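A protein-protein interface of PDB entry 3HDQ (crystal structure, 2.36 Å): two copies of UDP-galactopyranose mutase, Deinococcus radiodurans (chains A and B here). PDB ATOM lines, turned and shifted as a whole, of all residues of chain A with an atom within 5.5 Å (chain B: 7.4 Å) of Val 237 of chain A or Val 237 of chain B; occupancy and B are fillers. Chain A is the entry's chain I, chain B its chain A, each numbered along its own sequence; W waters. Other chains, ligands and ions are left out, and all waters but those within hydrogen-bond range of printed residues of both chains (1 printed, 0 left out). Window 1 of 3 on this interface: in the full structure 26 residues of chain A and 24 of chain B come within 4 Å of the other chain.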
ATOM      1  N   LEU A  56      -6.245 -31.828  15.782  1.00  0.00           N
ATOM      2  CA  LEU A  56      -6.925 -30.537  15.842  1.00  0.00           C
ATOM      3  C   LEU A  56      -8.263 -30.680  15.147  1.00  0.00           C
ATOM      4  O   LEU A  56      -8.314 -31.023  13.962  1.00  0.00           O
ATOM      5  CB  LEU A  56      -6.128 -29.440  15.139  1.00  0.00           C
ATOM      6  CG  LEU A  56      -6.868 -28.106  14.961  1.00  0.00           C
ATOM      7  CD1 LEU A  56      -7.216 -27.465  16.315  1.00  0.00           C
ATOM      8  CD2 LEU A  56      -6.073 -27.121  14.113  1.00  0.00           C
ATOM      9  N   ILE A  57      -9.351 -30.427  15.863  1.00  0.00           N
ATOM     10  CA  ILE A  57     -10.661 -30.506  15.230  1.00  0.00           C
ATOM     11  C   ILE A  57     -11.278 -29.121  15.142  1.00  0.00           C
ATOM     12  O   ILE A  57     -11.196 -28.327  16.077  1.00  0.00           O
ATOM     13  CB  ILE A  57     -11.597 -31.574  15.891  1.00  0.00           C
ATOM     14  CG1 ILE A  57     -12.932 -31.654  15.147  1.00  0.00           C
ATOM     15  CG2 ILE A  57     -11.792 -31.317  17.379  1.00  0.00           C
ATOM     16  CD1 ILE A  57     -13.730 -32.899  15.484  1.00  0.00           C
ATOM     17  N   ILE A  64     -19.715 -27.549  19.063  1.00  0.00           N
ATOM     18  CA  ILE A  64     -19.449 -28.900  18.590  1.00  0.00           C
ATOM     19  C   ILE A  64     -20.759 -29.653  18.324  1.00  0.00           C
ATOM     20  O   ILE A  64     -21.844 -29.080  18.464  1.00  0.00           O
ATOM     21  CB  ILE A  64     -18.577 -29.663  19.585  1.00  0.00           C
ATOM     22  CG1 ILE A  64     -19.409 -30.176  20.760  1.00  0.00           C
ATOM     23  CG2 ILE A  64     -17.476 -28.758  20.095  1.00  0.00           C
ATOM     24  CD1 ILE A  64     -18.580 -30.677  21.897  1.00  0.00           C
ATOM     25  N   LEU A 230     -14.756 -35.624  23.101  1.00  0.00           N
ATOM     26  CA  LEU A 230     -13.679 -34.749  22.662  1.00  0.00           C
ATOM     27  C   LEU A 230     -12.754 -34.295  23.791  1.00  0.00           C
ATOM     28  O   LEU A 230     -12.010 -33.330  23.628  1.00  0.00           O
ATOM     29  CB  LEU A 230     -14.262 -33.508  21.976  1.00  0.00           C
ATOM     30  CG  LEU A 230     -14.977 -33.694  20.634  1.00  0.00           C
ATOM     31  CD1 LEU A 230     -15.373 -32.357  20.077  1.00  0.00           C
ATOM     32  CD2 LEU A 230     -14.102 -34.429  19.634  1.00  0.00           C
ATOM     33  N   ILE A 235      -6.716 -33.761  21.957  1.00  0.00           N
ATOM     34  CA  ILE A 235      -7.697 -33.112  21.084  1.00  0.00           C
ATOM     35  C   ILE A 235      -7.827 -31.609  21.362  1.00  0.00           C
ATOM     36  O   ILE A 235      -8.234 -31.203  22.440  1.00  0.00           O
ATOM     37  CB  ILE A 235      -9.084 -33.766  21.212  1.00  0.00           C
ATOM     38  CG1 ILE A 235      -9.037 -35.226  20.730  1.00  0.00           C
ATOM     39  CG2 ILE A 235     -10.104 -32.971  20.419  1.00  0.00           C
ATOM     40  CD1 ILE A 235     -10.273 -36.041  21.075  1.00  0.00           C
ATOM     41  N   LYS A 236      -7.461 -30.785  20.391  1.00  0.00           N
ATOM     42  CA  LYS A 236      -7.684 -29.360  20.518  1.00  0.00           C
ATOM     43  C   LYS A 236      -8.848 -29.001  19.623  1.00  0.00           C
ATOM     44  O   LYS A 236      -8.937 -29.470  18.483  1.00  0.00           O
ATOM     45  CB  LYS A 236      -6.437 -28.567  20.118  1.00  0.00           C
ATOM     46  CG  LYS A 236      -5.169 -29.040  20.809  1.00  0.00           C
ATOM     47  CD  LYS A 236      -5.324 -29.030  22.316  1.00  0.00           C
ATOM     48  CE  LYS A 236      -4.193 -29.764  22.998  1.00  0.00           C
ATOM     49  NZ  LYS A 236      -4.486 -29.979  24.447  1.00  0.00           N
ATOM     50  N   VAL A 237      -9.746 -28.177  20.145  1.00  0.00           N
ATOM     51  CA  VAL A 237     -10.990 -27.860  19.454  1.00  0.00           C
ATOM     52  C   VAL A 237     -10.987 -26.391  19.058  1.00  0.00           C
ATOM     53  O   VAL A 237     -10.817 -25.506  19.904  1.00  0.00           O
ATOM     54  CB  VAL A 237     -12.214 -28.130  20.373  1.00  0.00           C
ATOM     55  CG1 VAL A 237     -13.506 -27.908  19.623  1.00  0.00           C
ATOM     56  CG2 VAL A 237     -12.147 -29.554  20.966  1.00  0.00           C
ATOM     57  N   MET A 238     -11.170 -26.125  17.775  1.00  0.00           N
ATOM     58  CA  MET A 238     -11.226 -24.755  17.302  1.00  0.00           C
ATOM     59  C   MET A 238     -12.582 -24.521  16.661  1.00  0.00           C
ATOM     60  O   MET A 238     -12.967 -25.205  15.711  1.00  0.00           O
ATOM     61  CB  MET A 238     -10.096 -24.490  16.309  1.00  0.00           C
ATOM     62  CG  MET A 238      -9.851 -23.029  16.010  1.00  0.00           C
ATOM     63  SD  MET A 238      -8.276 -22.831  15.148  1.00  0.00           S
ATOM     64  CE  MET A 238      -8.347 -21.105  14.733  1.00  0.00           C
ATOM     65  N   LEU A 239     -13.305 -23.552  17.202  1.00  0.00           N
ATOM     66  CA  LEU A 239     -14.678 -23.289  16.802  1.00  0.00           C
ATOM     67  C   LEU A 239     -14.793 -21.934  16.126  1.00  0.00           C
ATOM     68  O   LEU A 239     -13.869 -21.126  16.168  1.00  0.00           O
ATOM     69  CB  LEU A 239     -15.604 -23.341  18.022  1.00  0.00           C
ATOM     70  CG  LEU A 239     -15.687 -24.712  18.680  1.00  0.00           C
ATOM     71  CD1 LEU A 239     -16.599 -24.671  19.898  1.00  0.00           C
ATOM     72  CD2 LEU A 239     -16.191 -25.722  17.672  1.00  0.00           C
ATOM     73  N   ASN A 240     -15.951 -21.699  15.521  1.00  0.00           N
ATOM     74  CA  ASN A 240     -16.198 -20.499  14.746  1.00  0.00           C
ATOM     75  C   ASN A 240     -15.152 -20.345  13.647  1.00  0.00           C
ATOM     76  O   ASN A 240     -14.793 -19.233  13.263  1.00  0.00           O
ATOM     77  CB  ASN A 240     -16.236 -19.263  15.655  1.00  0.00           C
ATOM     78  CG  ASN A 240     -16.963 -18.102  15.012  1.00  0.00           C
ATOM     79  OD1 ASN A 240     -17.948 -18.303  14.299  1.00  0.00           O
ATOM     80  ND2 ASN A 240     -16.478 -16.882  15.244  1.00  0.00           N
ATOM     81  N   THR A 241     -14.682 -21.476  13.129  1.00  0.00           N
ATOM     82  CA  THR A 241     -13.504 -21.481  12.270  1.00  0.00           C
ATOM     83  C   THR A 241     -13.623 -22.314  10.989  1.00  0.00           C
ATOM     84  O   THR A 241     -13.794 -23.534  11.025  1.00  0.00           O
ATOM     85  CB  THR A 241     -12.264 -21.963  13.056  1.00  0.00           C
ATOM     86  OG1 THR A 241     -12.000 -21.058  14.137  1.00  0.00           O
ATOM     87  CG2 THR A 241     -11.054 -22.012  12.145  1.00  0.00           C
ATOM     88  N   ALA B  37     -10.304 -17.124  28.168  1.00  0.00           N
ATOM     89  CA  ALA B  37     -11.585 -16.636  27.657  1.00  0.00           C
ATOM     90  C   ALA B  37     -12.553 -16.201  28.773  1.00  0.00           C
ATOM     91  O   ALA B  37     -13.776 -16.317  28.635  1.00  0.00           O
ATOM     92  CB  ALA B  37     -12.233 -17.681  26.772  1.00  0.00           C
ATOM     93  N   VAL B  55      -8.391 -12.440  15.631  1.00  0.00           N
ATOM     94  CA  VAL B  55      -8.136 -12.898  16.980  1.00  0.00           C
ATOM     95  C   VAL B  55      -8.193 -14.420  17.102  1.00  0.00           C
ATOM     96  O   VAL B  55      -9.105 -15.057  16.596  1.00  0.00           O
ATOM     97  CB  VAL B  55      -9.130 -12.238  17.963  1.00  0.00           C
ATOM     98  CG1 VAL B  55      -8.886 -12.717  19.383  1.00  0.00           C
ATOM     99  CG2 VAL B  55      -9.006 -10.717  17.872  1.00  0.00           C
ATOM    100  N   LEU B  56      -7.188 -15.002  17.747  1.00  0.00           N
ATOM    101  CA  LEU B  56      -7.291 -16.374  18.195  1.00  0.00           C
ATOM    102  C   LEU B  56      -7.363 -16.312  19.704  1.00  0.00           C
ATOM    103  O   LEU B  56      -6.448 -15.790  20.354  1.00  0.00           O
ATOM    104  CB  LEU B  56      -6.084 -17.212  17.760  1.00  0.00           C
ATOM    105  CG  LEU B  56      -6.110 -18.652  18.287  1.00  0.00           C
ATOM    106  CD1 LEU B  56      -7.288 -19.414  17.701  1.00  0.00           C
ATOM    107  CD2 LEU B  56      -4.801 -19.381  18.001  1.00  0.00           C
ATOM    108  N   ILE B  57      -8.465 -16.806  20.263  1.00  0.00           N
ATOM    109  CA  ILE B  57      -8.596 -16.838  21.711  1.00  0.00           C
ATOM    110  C   ILE B  57      -8.522 -18.277  22.182  1.00  0.00           C
ATOM    111  O   ILE B  57      -9.196 -19.155  21.653  1.00  0.00           O
ATOM    112  CB  ILE B  57      -9.881 -16.125  22.220  1.00  0.00           C
ATOM    113  CG1 ILE B  57      -9.826 -15.962  23.746  1.00  0.00           C
ATOM    114  CG2 ILE B  57     -11.134 -16.882  21.796  1.00  0.00           C
ATOM    115  CD1 ILE B  57     -10.893 -15.013  24.329  1.00  0.00           C
ATOM    116  N   VAL B  58      -7.677 -18.522  23.171  1.00  0.00           N
ATOM    117  CA  VAL B  58      -7.439 -19.881  23.605  1.00  0.00           C
ATOM    118  C   VAL B  58      -7.714 -20.029  25.105  1.00  0.00           C
ATOM    119  O   VAL B  58      -7.527 -19.089  25.879  1.00  0.00           O
ATOM    120  CB  VAL B  58      -6.008 -20.308  23.229  1.00  0.00           C
ATOM    121  CG1 VAL B  58      -4.983 -19.662  24.158  1.00  0.00           C
ATOM    122  CG2 VAL B  58      -5.876 -21.813  23.247  1.00  0.00           C
ATOM    123  N   ASP B  59      -8.193 -21.199  25.513  1.00  0.00           N
ATOM    124  CA  ASP B  59      -8.305 -21.503  26.938  1.00  0.00           C
ATOM    125  C   ASP B  59      -8.016 -22.978  27.141  1.00  0.00           C
ATOM    126  O   ASP B  59      -8.422 -23.819  26.337  1.00  0.00           O
ATOM    127  CB  ASP B  59      -9.699 -21.136  27.468  1.00  0.00           C
ATOM    128  CG  ASP B  59      -9.722 -20.916  28.986  1.00  0.00           C
ATOM    129  OD1 ASP B  59      -9.407 -21.857  29.753  1.00  0.00           O
ATOM    130  OD2 ASP B  59     -10.079 -19.798  29.410  1.00  0.00           O
ATOM    131  N   PRO B  62     -12.311 -26.567  28.778  1.00  0.00           N
ATOM    132  CA  PRO B  62     -13.062 -26.997  27.590  1.00  0.00           C
ATOM    133  C   PRO B  62     -14.250 -26.098  27.317  1.00  0.00           C
ATOM    134  O   PRO B  62     -15.102 -26.464  26.520  1.00  0.00           O
ATOM    135  CB  PRO B  62     -13.583 -28.390  27.971  1.00  0.00           C
ATOM    136  CG  PRO B  62     -13.327 -28.537  29.483  1.00  0.00           C
ATOM    137  CD  PRO B  62     -12.774 -27.243  30.000  1.00  0.00           C
ATOM    138  N   HIS B  63     -14.311 -24.940  27.964  1.00  0.00           N
ATOM    139  CA  HIS B  63     -15.441 -24.032  27.789  1.00  0.00           C
ATOM    140  C   HIS B  63     -14.951 -22.593  27.868  1.00  0.00           C
ATOM    141  O   HIS B  63     -13.851 -22.349  28.347  1.00  0.00           O
ATOM    142  CB  HIS B  63     -16.468 -24.275  28.891  1.00  0.00           C
ATOM    143  CG  HIS B  63     -15.932 -24.008  30.263  1.00  0.00           C
ATOM    144  ND1 HIS B  63     -15.636 -22.739  30.707  1.00  0.00           N
ATOM    145  CD2 HIS B  63     -15.613 -24.848  31.278  1.00  0.00           C
ATOM    146  CE1 HIS B  63     -15.166 -22.805  31.942  1.00  0.00           C
ATOM    147  NE2 HIS B  63     -15.143 -24.073  32.311  1.00  0.00           N
ATOM    148  N   ILE B  64     -15.768 -21.648  27.408  1.00  0.00           N
ATOM    149  CA  ILE B  64     -15.445 -20.228  27.502  1.00  0.00           C
ATOM    150  C   ILE B  64     -15.910 -19.649  28.849  1.00  0.00           C
ATOM    151  O   ILE B  64     -16.486 -20.363  29.678  1.00  0.00           O
ATOM    152  CB  ILE B  64     -16.091 -19.425  26.343  1.00  0.00           C
ATOM    153  CG1 ILE B  64     -17.621 -19.531  26.407  1.00  0.00           C
ATOM    154  CG2 ILE B  64     -15.572 -19.927  24.998  1.00  0.00           C
ATOM    155  CD1 ILE B  64     -18.365 -18.763  25.334  1.00  0.00           C
ATOM    156  N   LEU B 230     -18.120 -13.407  21.755  1.00  0.00           N
ATOM    157  CA  LEU B 230     -17.100 -14.055  20.935  1.00  0.00           C
ATOM    158  C   LEU B 230     -17.643 -14.470  19.564  1.00  0.00           C
ATOM    159  O   LEU B 230     -17.026 -15.275  18.872  1.00  0.00           O
ATOM    160  CB  LEU B 230     -16.538 -15.277  21.671  1.00  0.00           C
ATOM    161  CG  LEU B 230     -16.000 -15.047  23.090  1.00  0.00           C
ATOM    162  CD1 LEU B 230     -15.483 -16.350  23.688  1.00  0.00           C
ATOM    163  CD2 LEU B 230     -14.909 -14.011  23.067  1.00  0.00           C
ATOM    164  N   SER B 231     -18.783 -13.913  19.169  1.00  0.00           N
ATOM    165  CA  SER B 231     -19.459 -14.355  17.949  1.00  0.00           C
ATOM    166  C   SER B 231     -18.883 -13.804  16.642  1.00  0.00           C
ATOM    167  O   SER B 231     -19.112 -14.383  15.578  1.00  0.00           O
ATOM    168  CB  SER B 231     -20.960 -14.032  18.012  1.00  0.00           C
ATOM    169  OG  SER B 231     -21.156 -12.633  18.053  1.00  0.00           O
ATOM    170  N   SER B 232     -18.172 -12.682  16.715  1.00  0.00           N
ATOM    171  CA  SER B 232     -17.610 -12.054  15.518  1.00  0.00           C
ATOM    172  C   SER B 232     -16.866 -13.050  14.625  1.00  0.00           C
ATOM    173  O   SER B 232     -16.190 -13.954  15.118  1.00  0.00           O
ATOM    174  CB  SER B 232     -16.663 -10.910  15.889  1.00  0.00           C
ATOM    175  OG  SER B 232     -15.841 -10.556  14.782  1.00  0.00           O
ATOM    176  N   ILE B 235     -13.145 -13.710  15.263  1.00  0.00           N
ATOM    177  CA  ILE B 235     -12.726 -14.377  16.490  1.00  0.00           C
ATOM    178  C   ILE B 235     -12.722 -15.901  16.326  1.00  0.00           C
ATOM    179  O   ILE B 235     -13.757 -16.509  16.070  1.00  0.00           O
ATOM    180  CB  ILE B 235     -13.613 -13.954  17.682  1.00  0.00           C
ATOM    181  CG1 ILE B 235     -13.513 -12.444  17.894  1.00  0.00           C
ATOM    182  CG2 ILE B 235     -13.189 -14.666  18.951  1.00  0.00           C
ATOM    183  CD1 ILE B 235     -14.240 -11.948  19.141  1.00  0.00           C
ATOM    184  N   LYS B 236     -11.542 -16.503  16.447  1.00  0.00           N
ATOM    185  CA  LYS B 236     -11.401 -17.955  16.425  1.00  0.00           C
ATOM    186  C   LYS B 236     -11.243 -18.427  17.859  1.00  0.00           C
ATOM    187  O   LYS B 236     -10.438 -17.873  18.613  1.00  0.00           O
ATOM    188  CB  LYS B 236     -10.179 -18.378  15.598  1.00  0.00           C
ATOM    189  CG  LYS B 236     -10.145 -17.807  14.186  1.00  0.00           C
ATOM    190  CD  LYS B 236     -11.450 -18.070  13.467  1.00  0.00           C
ATOM    191  CE  LYS B 236     -11.771 -16.937  12.518  1.00  0.00           C
ATOM    192  NZ  LYS B 236     -13.172 -16.992  12.015  1.00  0.00           N
ATOM    193  N   VAL B 237     -12.009 -19.445  18.239  1.00  0.00           N
ATOM    194  CA  VAL B 237     -12.025 -19.890  19.626  1.00  0.00           C
ATOM    195  C   VAL B 237     -11.460 -21.296  19.789  1.00  0.00           C
ATOM    196  O   VAL B 237     -11.996 -22.254  19.252  1.00  0.00           O
ATOM    197  CB  VAL B 237     -13.437 -19.865  20.188  1.00  0.00           C
ATOM    198  CG1 VAL B 237     -13.411 -20.178  21.679  1.00  0.00           C
ATOM    199  CG2 VAL B 237     -14.086 -18.516  19.914  1.00  0.00           C
ATOM    200  N   MET B 238     -10.383 -21.409  20.553  1.00  0.00           N
ATOM    201  CA  MET B 238      -9.686 -22.676  20.724  1.00  0.00           C
ATOM    202  C   MET B 238      -9.767 -23.156  22.177  1.00  0.00           C
ATOM    203  O   MET B 238      -9.234 -22.519  23.092  1.00  0.00           O
ATOM    204  CB  MET B 238      -8.230 -22.506  20.304  1.00  0.00           C
ATOM    205  CG  MET B 238      -7.534 -23.771  19.923  1.00  0.00           C
ATOM    206  SD  MET B 238      -5.946 -23.424  19.143  1.00  0.00           S
ATOM    207  CE  MET B 238      -5.576 -25.084  18.611  1.00  0.00           C
ATOM    208  N   LEU B 239     -10.441 -24.280  22.387  1.00  0.00           N
ATOM    209  CA  LEU B 239     -10.657 -24.787  23.733  1.00  0.00           C
ATOM    210  C   LEU B 239      -9.826 -26.037  24.013  1.00  0.00           C
ATOM    211  O   LEU B 239      -9.292 -26.656  23.096  1.00  0.00           O
ATOM    212  CB  LEU B 239     -12.158 -25.027  23.985  1.00  0.00           C
ATOM    213  CG  LEU B 239     -13.018 -23.759  23.831  1.00  0.00           C
ATOM    214  CD1 LEU B 239     -14.479 -24.016  24.137  1.00  0.00           C
ATOM    215  CD2 LEU B 239     -12.489 -22.645  24.716  1.00  0.00           C
ATOM    216  N   ASN B 240      -9.725 -26.401  25.286  1.00  0.00           N
ATOM    217  CA  ASN B 240      -8.930 -27.540  25.700  1.00  0.00           C
ATOM    218  C   ASN B 240      -7.460 -27.367  25.304  1.00  0.00           C
ATOM    219  O   ASN B 240      -6.765 -28.339  24.998  1.00  0.00           O
ATOM    220  CB  ASN B 240      -9.497 -28.829  25.102  1.00  0.00           C
ATOM    221  CG  ASN B 240      -9.204 -30.038  25.969  1.00  0.00           C
ATOM    222  OD1 ASN B 240      -9.199 -29.936  27.196  1.00  0.00           O
ATOM    223  ND2 ASN B 240      -8.950 -31.188  25.340  1.00  0.00           N
ATOM    224  N   THR B 241      -6.994 -26.123  25.330  1.00  0.00           N
ATOM    225  CA  THR B 241      -5.688 -25.781  24.768  1.00  0.00           C
ATOM    226  C   THR B 241      -4.847 -24.818  25.620  1.00  0.00           C
ATOM    227  O   THR B 241      -5.153 -23.640  25.728  1.00  0.00           O
ATOM    228  CB  THR B 241      -5.858 -25.181  23.361  1.00  0.00           C
ATOM    229  OG1 THR B 241      -6.596 -26.092  22.533  1.00  0.00           O
ATOM    230  CG2 THR B 241      -4.506 -24.889  22.733  1.00  0.00           C
HETATM  231  O   HOH W   1     -20.035 -16.763  15.615  1.00  0.00           O
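Water W1 lies within hydrogen-bond range of O of Ser 231 of chain B (2.6 Å) and OD1 of Asn 240 of chain A (2.9 Å).
The backbone NH of Leu 239 of chain A sits at hydrogen-bond distance from the backbone carbonyl oxygen of Val 237 of chain B (2.8 Å). The backbone carbonyl oxygen (O) of Ile 235 of chain A lies within hydrogen-bond range of the side-chain amide nitrogen (ND2) of Asn 240 of chain B. The side-chain amino group of Lys 236 of chain B is in hydrogen-bond range of the backbone carbonyl oxygen of Asn 240 of chain A (3.0 Å). NZ of Lys 236 of chain A lies within hydrogen-bond range of O of Asn 240 of chain B (2.9 Å). ND2 of Asn 240 of chain A is in hydrogen-bond range of O of Ser 232 of chain B (2.9 Å). The backbone carbonyl oxygen of Ile 235 of chain B sits at hydrogen-bond distance from the side-chain amide nitrogen of Asn 240 of chain A, 2.9 Å away. The backbone NH (N) of Leu 239 of chain B is in hydrogen-bond range of the backbone carbonyl oxygen (O) of Val 237 of chain A (2.8 Å).
The backbone NH of Ile 57 of chain B sits at hydrogen-bond distance from the backbone carbonyl oxygen of Lys 236 of chain B (2.8 Å). O of Val 55 of chain B is in hydrogen-bond range of N of Lys 236 of chain B (2.8 Å). The side-chain hydroxyl of Thr 241 of chain B sits at hydrogen-bond distance from the backbone carbonyl oxygen of Leu 239 of chain B, 2.8 Å away. The backbone carbonyl oxygen of Asp 59 of chain B lies within hydrogen-bond range of the backbone NH of Thr 241 of chain B. The backbone carbonyl oxygen of Ile 57 of chain A is in hydrogen-bond range of the backbone NH of Met 238 of chain A (2.8 Å). The backbone carbonyl oxygen (O) of Leu 239 of chain A sits at hydrogen-bond distance from the side-chain hydroxyl (OG1) of Thr 241 of chain A (2.8 Å).
Printed residues of chain B within 4 Å of Met 238 of chain A: Leu 56, Lys 236 and Val 237. Printed residues of chain A within 4 Å of Ser 232 of chain B: Asn 240 (2.9 Å). Printed residues of chain A within 4 Å of Ile 235 of chain B: Asn 240. Val 237 of chain B touches three residues of chain A. Printed residues of chain A within 4 Å of Leu 239 of chain B: Val 237 (2.8 Å). The nearest residue of chain B that does not touch Val 237 of chain A is Thr 241 of chain B (4.5 Å). The nearest printed residue of chain A that does not touch Ser 232 of chain B is Leu 239 of chain A (7.6 Å).
CD1 of Leu 56 of chain A touches CE of Met 238 of chain B (3.7 Å). Lys 236 of chain A touches Met 238 of chain B. Lys 236 of chain A touches Thr 241 of chain B (CD to OG1, 3.2 Å). Val 237 of chain A touches Val 237 of chain B (O to O, 3.5 Å). Val 237 of chain A touches Met 238 of chain B (O to CA, 3.2 Å). Met 238 of chain A touches Leu 56 of chain B (CE to CD1, 3.6 Å). Met 238 of chain A touches Lys 236 of chain B (CE to CB, 3.4 Å). Met 238 of chain A touches Val 237 of chain B. Ser 231 of chain B touches Asn 240 of chain A. CD of Lys 236 of chain B touches OG1 of Thr 241 of chain A (3.1 Å).
Lys 236 of chain A touches Met 238 of chain B, and with the chains exchanged Met 238 of chain A touches Lys 236 of chain B. Lys 236 of chain A touches Thr 241 of chain B, and with the chains exchanged Thr 241 of chain A touches Lys 236 of chain B. Val 237 of chain B touches its own counterpart, Val 237 of chain A. Val 237 of chain A touches Leu 239 of chain B, and with the chains exchanged Leu 239 of chain A touches Val 237 of chain B. 11 positions are printed for both chains. Of the 17 pairs that touch across the chains among the printed residues, 15 have their exchanged pair printed and touching as well.
Of the 19 printed residues of chain B, 10 touch a printed residue of chain A. Printed residues of chain B that touch a printed residue of chain A: Leu 56, Ser 231, Ser 232, Ile 235, Lys 236, Val 237, Met 238, Leu 239, Asn 240 and Thr 241. Hydrophobic or aromatic side chains of chain B that line the printed part of chain A: Leu 56 and Met 238. Among the printed residues, 17 pairs touch across the chains.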
